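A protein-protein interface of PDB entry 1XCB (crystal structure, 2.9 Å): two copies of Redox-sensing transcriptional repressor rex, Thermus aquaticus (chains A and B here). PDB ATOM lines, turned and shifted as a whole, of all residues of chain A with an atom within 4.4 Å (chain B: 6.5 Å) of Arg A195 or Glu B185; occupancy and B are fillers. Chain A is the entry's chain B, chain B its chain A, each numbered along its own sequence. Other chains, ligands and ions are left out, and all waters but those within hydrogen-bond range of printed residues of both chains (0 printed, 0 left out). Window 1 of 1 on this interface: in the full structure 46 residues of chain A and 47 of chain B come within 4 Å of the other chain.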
ATOM      1  N   ALA A 191       9.912   6.530  35.872  1.00  0.00           N
ATOM      2  CA  ALA A 191      10.467   5.377  35.159  1.00  0.00           C
ATOM      3  C   ALA A 191      10.207   5.417  33.651  1.00  0.00           C
ATOM      4  O   ALA A 191      11.097   5.089  32.858  1.00  0.00           O
ATOM      5  CB  ALA A 191       9.937   4.095  35.748  1.00  0.00           C
ATOM      6  N   GLY A 192       9.004   5.825  33.251  1.00  0.00           N
ATOM      7  CA  GLY A 192       8.704   5.910  31.830  1.00  0.00           C
ATOM      8  C   GLY A 192       9.585   6.941  31.131  1.00  0.00           C
ATOM      9  O   GLY A 192       9.877   6.822  29.945  1.00  0.00           O
ATOM     10  N   LEU A 193      10.005   7.964  31.869  1.00  0.00           N
ATOM     11  CA  LEU A 193      10.865   9.009  31.316  1.00  0.00           C
ATOM     12  C   LEU A 193      12.195   8.420  30.844  1.00  0.00           C
ATOM     13  O   LEU A 193      12.664   8.722  29.737  1.00  0.00           O
ATOM     14  CB  LEU A 193      11.146  10.077  32.374  1.00  0.00           C
ATOM     15  CG  LEU A 193      10.686  11.507  32.113  1.00  0.00           C
ATOM     16  CD1 LEU A 193      11.220  12.391  33.207  1.00  0.00           C
ATOM     17  CD2 LEU A 193      11.195  11.999  30.780  1.00  0.00           C
ATOM     18  N   THR A 194      12.800   7.584  31.691  1.00  0.00           N
ATOM     19  CA  THR A 194      14.079   6.959  31.364  1.00  0.00           C
ATOM     20  C   THR A 194      13.880   5.923  30.279  1.00  0.00           C
ATOM     21  O   THR A 194      14.742   5.730  29.433  1.00  0.00           O
ATOM     22  CB  THR A 194      14.699   6.265  32.576  1.00  0.00           C
ATOM     23  OG1 THR A 194      14.721   7.162  33.692  1.00  0.00           O
ATOM     24  CG2 THR A 194      16.112   5.856  32.260  1.00  0.00           C
ATOM     25  N   ARG A 195      12.746   5.234  30.314  1.00  0.00           N
ATOM     26  CA  ARG A 195      12.477   4.257  29.273  1.00  0.00           C
ATOM     27  C   ARG A 195      12.440   5.047  27.981  1.00  0.00           C
ATOM     28  O   ARG A 195      12.796   4.539  26.922  1.00  0.00           O
ATOM     29  CB  ARG A 195      11.133   3.576  29.482  1.00  0.00           C
ATOM     30  CG  ARG A 195      11.190   2.367  30.360  1.00  0.00           C
ATOM     31  CD  ARG A 195       9.937   1.546  30.159  1.00  0.00           C
ATOM     32  NE  ARG A 195       8.834   2.038  30.966  1.00  0.00           N
ATOM     33  CZ  ARG A 195       8.678   1.754  32.254  1.00  0.00           C
ATOM     34  NH1 ARG A 195       9.562   0.976  32.870  1.00  0.00           N
ATOM     35  NH2 ARG A 195       7.643   2.247  32.926  1.00  0.00           N
ATOM     36  N   LEU A 196      11.999   6.301  28.093  1.00  0.00           N
ATOM     37  CA  LEU A 196      11.908   7.209  26.954  1.00  0.00           C
ATOM     38  C   LEU A 196      13.337   7.542  26.576  1.00  0.00           C
ATOM     39  O   LEU A 196      13.755   7.360  25.424  1.00  0.00           O
ATOM     40  CB  LEU A 196      11.161   8.488  27.348  1.00  0.00           C
ATOM     41  CG  LEU A 196      10.786   9.440  26.206  1.00  0.00           C
ATOM     42  CD1 LEU A 196      10.003   8.668  25.155  1.00  0.00           C
ATOM     43  CD2 LEU A 196       9.964  10.610  26.730  1.00  0.00           C
ATOM     44  N   SER A 197      14.083   8.009  27.574  1.00  0.00           N
ATOM     45  CA  SER A 197      15.485   8.371  27.403  1.00  0.00           C
ATOM     46  C   SER A 197      16.240   7.290  26.638  1.00  0.00           C
ATOM     47  O   SER A 197      16.792   7.532  25.570  1.00  0.00           O
ATOM     48  CB  SER A 197      16.126   8.571  28.768  1.00  0.00           C
ATOM     49  OG  SER A 197      17.491   8.911  28.636  1.00  0.00           O
ATOM     50  N   PHE A 198      16.244   6.091  27.204  1.00  0.00           N
ATOM     51  CA  PHE A 198      16.911   4.942  26.609  1.00  0.00           C
ATOM     52  C   PHE A 198      16.371   4.608  25.214  1.00  0.00           C
ATOM     53  O   PHE A 198      17.122   4.234  24.319  1.00  0.00           O
ATOM     54  CB  PHE A 198      16.736   3.720  27.515  1.00  0.00           C
ATOM     55  CG  PHE A 198      17.336   2.468  26.951  1.00  0.00           C
ATOM     56  CD1 PHE A 198      18.684   2.184  27.135  1.00  0.00           C
ATOM     57  CD2 PHE A 198      16.580   1.627  26.143  1.00  0.00           C
ATOM     58  CE1 PHE A 198      19.271   1.090  26.514  1.00  0.00           C
ATOM     59  CE2 PHE A 198      17.158   0.537  25.520  1.00  0.00           C
ATOM     60  CZ  PHE A 198      18.507   0.269  25.702  1.00  0.00           C
ATOM     61  N   ALA A 199      15.063   4.742  25.044  1.00  0.00           N
ATOM     62  CA  ALA A 199      14.410   4.429  23.777  1.00  0.00           C
ATOM     63  C   ALA A 199      14.831   5.350  22.644  1.00  0.00           C
ATOM     64  O   ALA A 199      14.841   4.946  21.479  1.00  0.00           O
ATOM     65  CB  ALA A 199      12.905   4.488  23.948  1.00  0.00           C
ATOM     66  N   GLU B   5      12.344  -5.702  27.096  1.00  0.00           N
ATOM     67  CA  GLU B   5      11.825  -4.443  27.581  1.00  0.00           C
ATOM     68  C   GLU B   5      11.888  -4.459  29.102  1.00  0.00           C
ATOM     69  O   GLU B   5      12.202  -3.449  29.732  1.00  0.00           O
ATOM     70  CB  GLU B   5      10.384  -4.252  27.109  1.00  0.00           C
ATOM     71  CG  GLU B   5      10.212  -3.106  26.122  1.00  0.00           C
ATOM     72  CD  GLU B   5       9.535  -1.880  26.734  1.00  0.00           C
ATOM     73  OE1 GLU B   5       9.801  -1.555  27.919  1.00  0.00           O
ATOM     74  OE2 GLU B   5       8.741  -1.235  26.012  1.00  0.00           O
ATOM     75  N   ILE B   8      15.371  -3.295  30.689  1.00  0.00           N
ATOM     76  CA  ILE B   8      15.629  -1.865  30.803  1.00  0.00           C
ATOM     77  C   ILE B   8      14.867  -1.294  32.004  1.00  0.00           C
ATOM     78  O   ILE B   8      15.311  -0.335  32.640  1.00  0.00           O
ATOM     79  CB  ILE B   8      15.193  -1.096  29.515  1.00  0.00           C
ATOM     80  CG1 ILE B   8      16.343  -1.013  28.506  1.00  0.00           C
ATOM     81  CG2 ILE B   8      14.826   0.341  29.856  1.00  0.00           C
ATOM     82  CD1 ILE B   8      16.923  -2.338  28.046  1.00  0.00           C
ATOM     83  N   SER B   9      13.720  -1.886  32.317  1.00  0.00           N
ATOM     84  CA  SER B   9      12.932  -1.398  33.434  1.00  0.00           C
ATOM     85  C   SER B   9      13.568  -1.783  34.746  1.00  0.00           C
ATOM     86  O   SER B   9      13.450  -1.063  35.731  1.00  0.00           O
ATOM     87  CB  SER B   9      11.520  -1.958  33.375  1.00  0.00           C
ATOM     88  OG  SER B   9      10.868  -1.536  32.196  1.00  0.00           O
ATOM     89  N   ARG B  10      14.228  -2.933  34.766  1.00  0.00           N
ATOM     90  CA  ARG B  10      14.886  -3.396  35.982  1.00  0.00           C
ATOM     91  C   ARG B  10      16.120  -2.535  36.178  1.00  0.00           C
ATOM     92  O   ARG B  10      16.428  -2.129  37.297  1.00  0.00           O
ATOM     93  CB  ARG B  10      15.300  -4.866  35.862  1.00  0.00           C
ATOM     94  CG  ARG B  10      14.197  -5.860  36.090  1.00  0.00           C
ATOM     95  CD  ARG B  10      14.775  -7.259  36.220  1.00  0.00           C
ATOM     96  NE  ARG B  10      15.183  -7.816  34.934  1.00  0.00           N
ATOM     97  CZ  ARG B  10      14.347  -8.355  34.042  1.00  0.00           C
ATOM     98  NH1 ARG B  10      13.041  -8.422  34.288  1.00  0.00           N
ATOM     99  NH2 ARG B  10      14.821  -8.835  32.897  1.00  0.00           N
ATOM    100  N   ILE B  12      16.528   0.444  35.222  1.00  0.00           N
ATOM    101  CA  ILE B  12      15.999   1.689  35.739  1.00  0.00           C
ATOM    102  C   ILE B  12      15.794   1.589  37.255  1.00  0.00           C
ATOM    103  O   ILE B  12      15.936   2.580  37.967  1.00  0.00           O
ATOM    104  CB  ILE B  12      14.641   2.008  35.088  1.00  0.00           C
ATOM    105  CG1 ILE B  12      14.843   2.360  33.621  1.00  0.00           C
ATOM    106  CG2 ILE B  12      13.965   3.151  35.813  1.00  0.00           C
ATOM    107  CD1 ILE B  12      13.556   2.502  32.853  1.00  0.00           C
ATOM    108  N   LEU B  75      21.351   3.828  30.401  1.00  0.00           N
ATOM    109  CA  LEU B  75      20.018   4.347  30.195  1.00  0.00           C
ATOM    110  C   LEU B  75      20.004   5.727  29.553  1.00  0.00           C
ATOM    111  O   LEU B  75      18.953   6.375  29.462  1.00  0.00           O
ATOM    112  CB  LEU B  75      19.281   4.355  31.530  1.00  0.00           C
ATOM    113  CG  LEU B  75      19.124   2.951  32.114  1.00  0.00           C
ATOM    114  CD1 LEU B  75      18.531   3.055  33.506  1.00  0.00           C
ATOM    115  CD2 LEU B  75      18.245   2.093  31.203  1.00  0.00           C
ATOM    116  N   PHE B 105      16.973  15.288  33.924  1.00  0.00           N
ATOM    117  CA  PHE B 105      15.764  15.752  33.257  1.00  0.00           C
ATOM    118  C   PHE B 105      15.448  17.135  33.765  1.00  0.00           C
ATOM    119  O   PHE B 105      15.395  17.349  34.975  1.00  0.00           O
ATOM    120  CB  PHE B 105      14.597  14.819  33.551  1.00  0.00           C
ATOM    121  CG  PHE B 105      14.776  13.442  32.995  1.00  0.00           C
ATOM    122  CD1 PHE B 105      15.022  12.365  33.835  1.00  0.00           C
ATOM    123  CD2 PHE B 105      14.715  13.227  31.629  1.00  0.00           C
ATOM    124  CE1 PHE B 105      15.202  11.095  33.323  1.00  0.00           C
ATOM    125  CE2 PHE B 105      14.893  11.964  31.103  1.00  0.00           C
ATOM    126  CZ  PHE B 105      15.138  10.891  31.954  1.00  0.00           C
ATOM    127  N   GLY B 167      11.479  12.894  22.062  1.00  0.00           N
ATOM    128  CA  GLY B 167      10.617  11.856  22.591  1.00  0.00           C
ATOM    129  C   GLY B 167       9.373  12.385  23.266  1.00  0.00           C
ATOM    130  O   GLY B 167       9.359  13.501  23.792  1.00  0.00           O
ATOM    131  N   ILE B 168       8.326  11.567  23.268  1.00  0.00           N
ATOM    132  CA  ILE B 168       7.071  11.972  23.872  1.00  0.00           C
ATOM    133  C   ILE B 168       6.573  11.059  24.983  1.00  0.00           C
ATOM    134  O   ILE B 168       6.292   9.883  24.745  1.00  0.00           O
ATOM    135  CB  ILE B 168       5.959  12.052  22.814  1.00  0.00           C
ATOM    136  CG1 ILE B 168       6.400  12.951  21.656  1.00  0.00           C
ATOM    137  CG2 ILE B 168       4.696  12.600  23.452  1.00  0.00           C
ATOM    138  CD1 ILE B 168       5.327  13.192  20.601  1.00  0.00           C
ATOM    139  N   LEU B 169       6.476  11.599  26.195  1.00  0.00           N
ATOM    140  CA  LEU B 169       5.943  10.848  27.334  1.00  0.00           C
ATOM    141  C   LEU B 169       4.482  11.256  27.262  1.00  0.00           C
ATOM    142  O   LEU B 169       4.119  12.372  27.635  1.00  0.00           O
ATOM    143  CB  LEU B 169       6.549  11.331  28.648  1.00  0.00           C
ATOM    144  CG  LEU B 169       6.123  10.523  29.871  1.00  0.00           C
ATOM    145  CD1 LEU B 169       6.529   9.074  29.684  1.00  0.00           C
ATOM    146  CD2 LEU B 169       6.766  11.085  31.114  1.00  0.00           C
ATOM    147  N   ASN B 170       3.641  10.354  26.782  1.00  0.00           N
ATOM    148  CA  ASN B 170       2.233  10.668  26.573  1.00  0.00           C
ATOM    149  C   ASN B 170       1.197  10.163  27.579  1.00  0.00           C
ATOM    150  O   ASN B 170       0.971   8.959  27.711  1.00  0.00           O
ATOM    151  CB  ASN B 170       1.892  10.215  25.157  1.00  0.00           C
ATOM    152  CG  ASN B 170       0.458   9.849  24.995  1.00  0.00           C
ATOM    153  OD1 ASN B 170      -0.430  10.704  25.063  1.00  0.00           O
ATOM    154  ND2 ASN B 170       0.212   8.563  24.774  1.00  0.00           N
ATOM    155  N   PHE B 171       0.544  11.102  28.259  1.00  0.00           N
ATOM    156  CA  PHE B 171      -0.457  10.767  29.267  1.00  0.00           C
ATOM    157  C   PHE B 171      -1.890  10.625  28.755  1.00  0.00           C
ATOM    158  O   PHE B 171      -2.762  10.158  29.497  1.00  0.00           O
ATOM    159  CB  PHE B 171      -0.476  11.818  30.376  1.00  0.00           C
ATOM    160  CG  PHE B 171       0.807  11.932  31.148  1.00  0.00           C
ATOM    161  CD1 PHE B 171       1.941  12.495  30.570  1.00  0.00           C
ATOM    162  CD2 PHE B 171       0.858  11.554  32.484  1.00  0.00           C
ATOM    163  CE1 PHE B 171       3.105  12.688  31.316  1.00  0.00           C
ATOM    164  CE2 PHE B 171       2.012  11.742  33.234  1.00  0.00           C
ATOM    165  CZ  PHE B 171       3.136  12.313  32.648  1.00  0.00           C
ATOM    166  N   ALA B 183      10.398   8.848  19.664  1.00  0.00           N
ATOM    167  CA  ALA B 183       9.893   7.838  20.582  1.00  0.00           C
ATOM    168  C   ALA B 183       8.718   8.294  21.430  1.00  0.00           C
ATOM    169  O   ALA B 183       8.645   9.450  21.862  1.00  0.00           O
ATOM    170  CB  ALA B 183      11.020   7.360  21.490  1.00  0.00           C
ATOM    171  N   VAL B 184       7.805   7.359  21.670  1.00  0.00           N
ATOM    172  CA  VAL B 184       6.629   7.620  22.485  1.00  0.00           C
ATOM    173  C   VAL B 184       6.548   6.620  23.639  1.00  0.00           C
ATOM    174  O   VAL B 184       6.653   5.409  23.442  1.00  0.00           O
ATOM    175  CB  VAL B 184       5.325   7.512  21.663  1.00  0.00           C
ATOM    176  CG1 VAL B 184       4.161   7.991  22.494  1.00  0.00           C
ATOM    177  CG2 VAL B 184       5.434   8.324  20.395  1.00  0.00           C
ATOM    178  N   GLU B 185       6.382   7.151  24.842  1.00  0.00           N
ATOM    179  CA  GLU B 185       6.251   6.343  26.047  1.00  0.00           C
ATOM    180  C   GLU B 185       4.938   6.764  26.701  1.00  0.00           C
ATOM    181  O   GLU B 185       4.749   7.937  27.045  1.00  0.00           O
ATOM    182  CB  GLU B 185       7.411   6.604  27.005  1.00  0.00           C
ATOM    183  CG  GLU B 185       7.251   5.896  28.345  1.00  0.00           C
ATOM    184  CD  GLU B 185       7.435   4.383  28.258  1.00  0.00           C
ATOM    185  OE1 GLU B 185       7.066   3.693  29.231  1.00  0.00           O
ATOM    186  OE2 GLU B 185       7.955   3.884  27.234  1.00  0.00           O
ATOM    187  N   ASN B 186       4.036   5.809  26.876  1.00  0.00           N
ATOM    188  CA  ASN B 186       2.736   6.105  27.452  1.00  0.00           C
ATOM    189  C   ASN B 186       2.656   5.861  28.938  1.00  0.00           C
ATOM    190  O   ASN B 186       3.069   4.816  29.425  1.00  0.00           O
ATOM    191  CB  ASN B 186       1.683   5.283  26.740  1.00  0.00           C
ATOM    192  CG  ASN B 186       1.804   5.392  25.248  1.00  0.00           C
ATOM    193  OD1 ASN B 186       1.604   6.468  24.672  1.00  0.00           O
ATOM    194  ND2 ASN B 186       2.153   4.283  24.604  1.00  0.00           N
ATOM    195  N   VAL B 187       2.114   6.842  29.650  1.00  0.00           N
ATOM    196  CA  VAL B 187       1.956   6.760  31.095  1.00  0.00           C
ATOM    197  C   VAL B 187       0.599   6.146  31.456  1.00  0.00           C
ATOM    198  O   VAL B 187      -0.367   6.248  30.698  1.00  0.00           O
ATOM    199  CB  VAL B 187       2.069   8.158  31.728  1.00  0.00           C
ATOM    200  CG1 VAL B 187       1.839   8.078  33.213  1.00  0.00           C
ATOM    201  CG2 VAL B 187       3.440   8.737  31.447  1.00  0.00           C
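The side-chain carboxylate (OE1) of Glu B185 is in salt-bridge range of the guanidinium group (NE) of Arg A195, at 3.0 Å. O of Leu B75 lies within hydrogen-bond range of OG of Ser A197. The side-chain hydroxyl (OG) of Ser B9 sits at hydrogen-bond distance from the guanidinium group (NH1) of Arg A195 (2.9 Å).
O of Ile B168 sits at hydrogen-bond distance from N of Glu B185 (2.7 Å). The backbone NH (N) of Ile B168 lies within hydrogen-bond range of the backbone carbonyl oxygen (O) of Ala B183 (2.6 Å). The backbone carbonyl oxygen of Glu B5 lies within hydrogen-bond range of the side-chain hydroxyl of Ser B9 (3.4 Å). The backbone carbonyl oxygen (O) of Glu B185 is in hydrogen-bond range of the backbone NH (N) of Asn B170.
O of Ala A191 touches CD1 of Ile B12 (3.6 Å). C of Gly A192 touches CD1 of Leu B169 (3.998 Å). CG of Glu B185 touches O of Gly A192 (3.2 Å). Thr A194 touches Ile B12 (CB to CD1, 3.9 Å). Thr A194 touches Phe B105 (OG1 to CE1, 3.98 Å). Arg A195 touches Glu B5. Leu A196 touches Gly B167 (CD2 to C, 3.9 Å). Leu B169 touches Leu A196. Ala B183 touches Leu A196 (O to CD1, 3.6 Å). Phe A198 touches Leu B75 (N to O, 3.5 Å).
Of the printed residues of chain B, Arg A195 touches Glu B5, Ser B9, Ile B12 and Glu B185. Of chain A, only Gly A192 (3.2 Å), Arg A195 (3.0 Å) and Leu A196 (3.8 Å) come within 4 Å of Glu B185. Of the printed residues of chain A, Glu B5 touches Arg A195. Of the printed residues of chain A, Ala B183 touches Leu A196. Printed residues of chain A within 4 Å of Ile B12: Ala A191, Thr A194 and Arg A195. Of the printed residues of chain B, Leu A196 touches Gly B167 (3.9 Å), Ile B168 (3.8 Å), Leu B169 (3.7 Å), Ala B183 (3.6 Å) and Glu B185 (3.8 Å). Of the printed residues of chain B, Thr A194 touches Ile B12 (3.9 Å), Leu B75 (3.6 Å) and Phe B105 (3.98 Å). The nearest printed residue of chain A that does not touch Gly B167 is Ser A197 (7.2 Å).
Of the 17 printed residues of chain B, 11 touch a printed residue of chain A. Printed residues of chain B that touch a printed residue of chain A: Glu B5, Ile B8, Ser B9, Ile B12, Leu B75, Phe B105, Gly B167, Ile B168, Leu B169, Ala B183 and Glu B185. Hydrophobic or aromatic side chains of chain B that line the printed part of chain A: Ile B8, Ile B12, Leu B75, Phe B105 and Leu B169. Printed residues of chain A that touch a printed residue of chain B: Ala A191, Gly A192, Leu A193, Thr A194, Arg A195, Leu A196, Ser A197 and Phe A198. Hydrophobic or aromatic side chains of chain A that line the printed part of chain B: Leu A193, Leu A196 and Phe A198. Among the printed residues, Asp or Glu carboxylates within 4 Å of a Lys or Arg side-chain nitrogen of the other chain: Arg A195 with Glu B185.
No position is printed for both chains.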
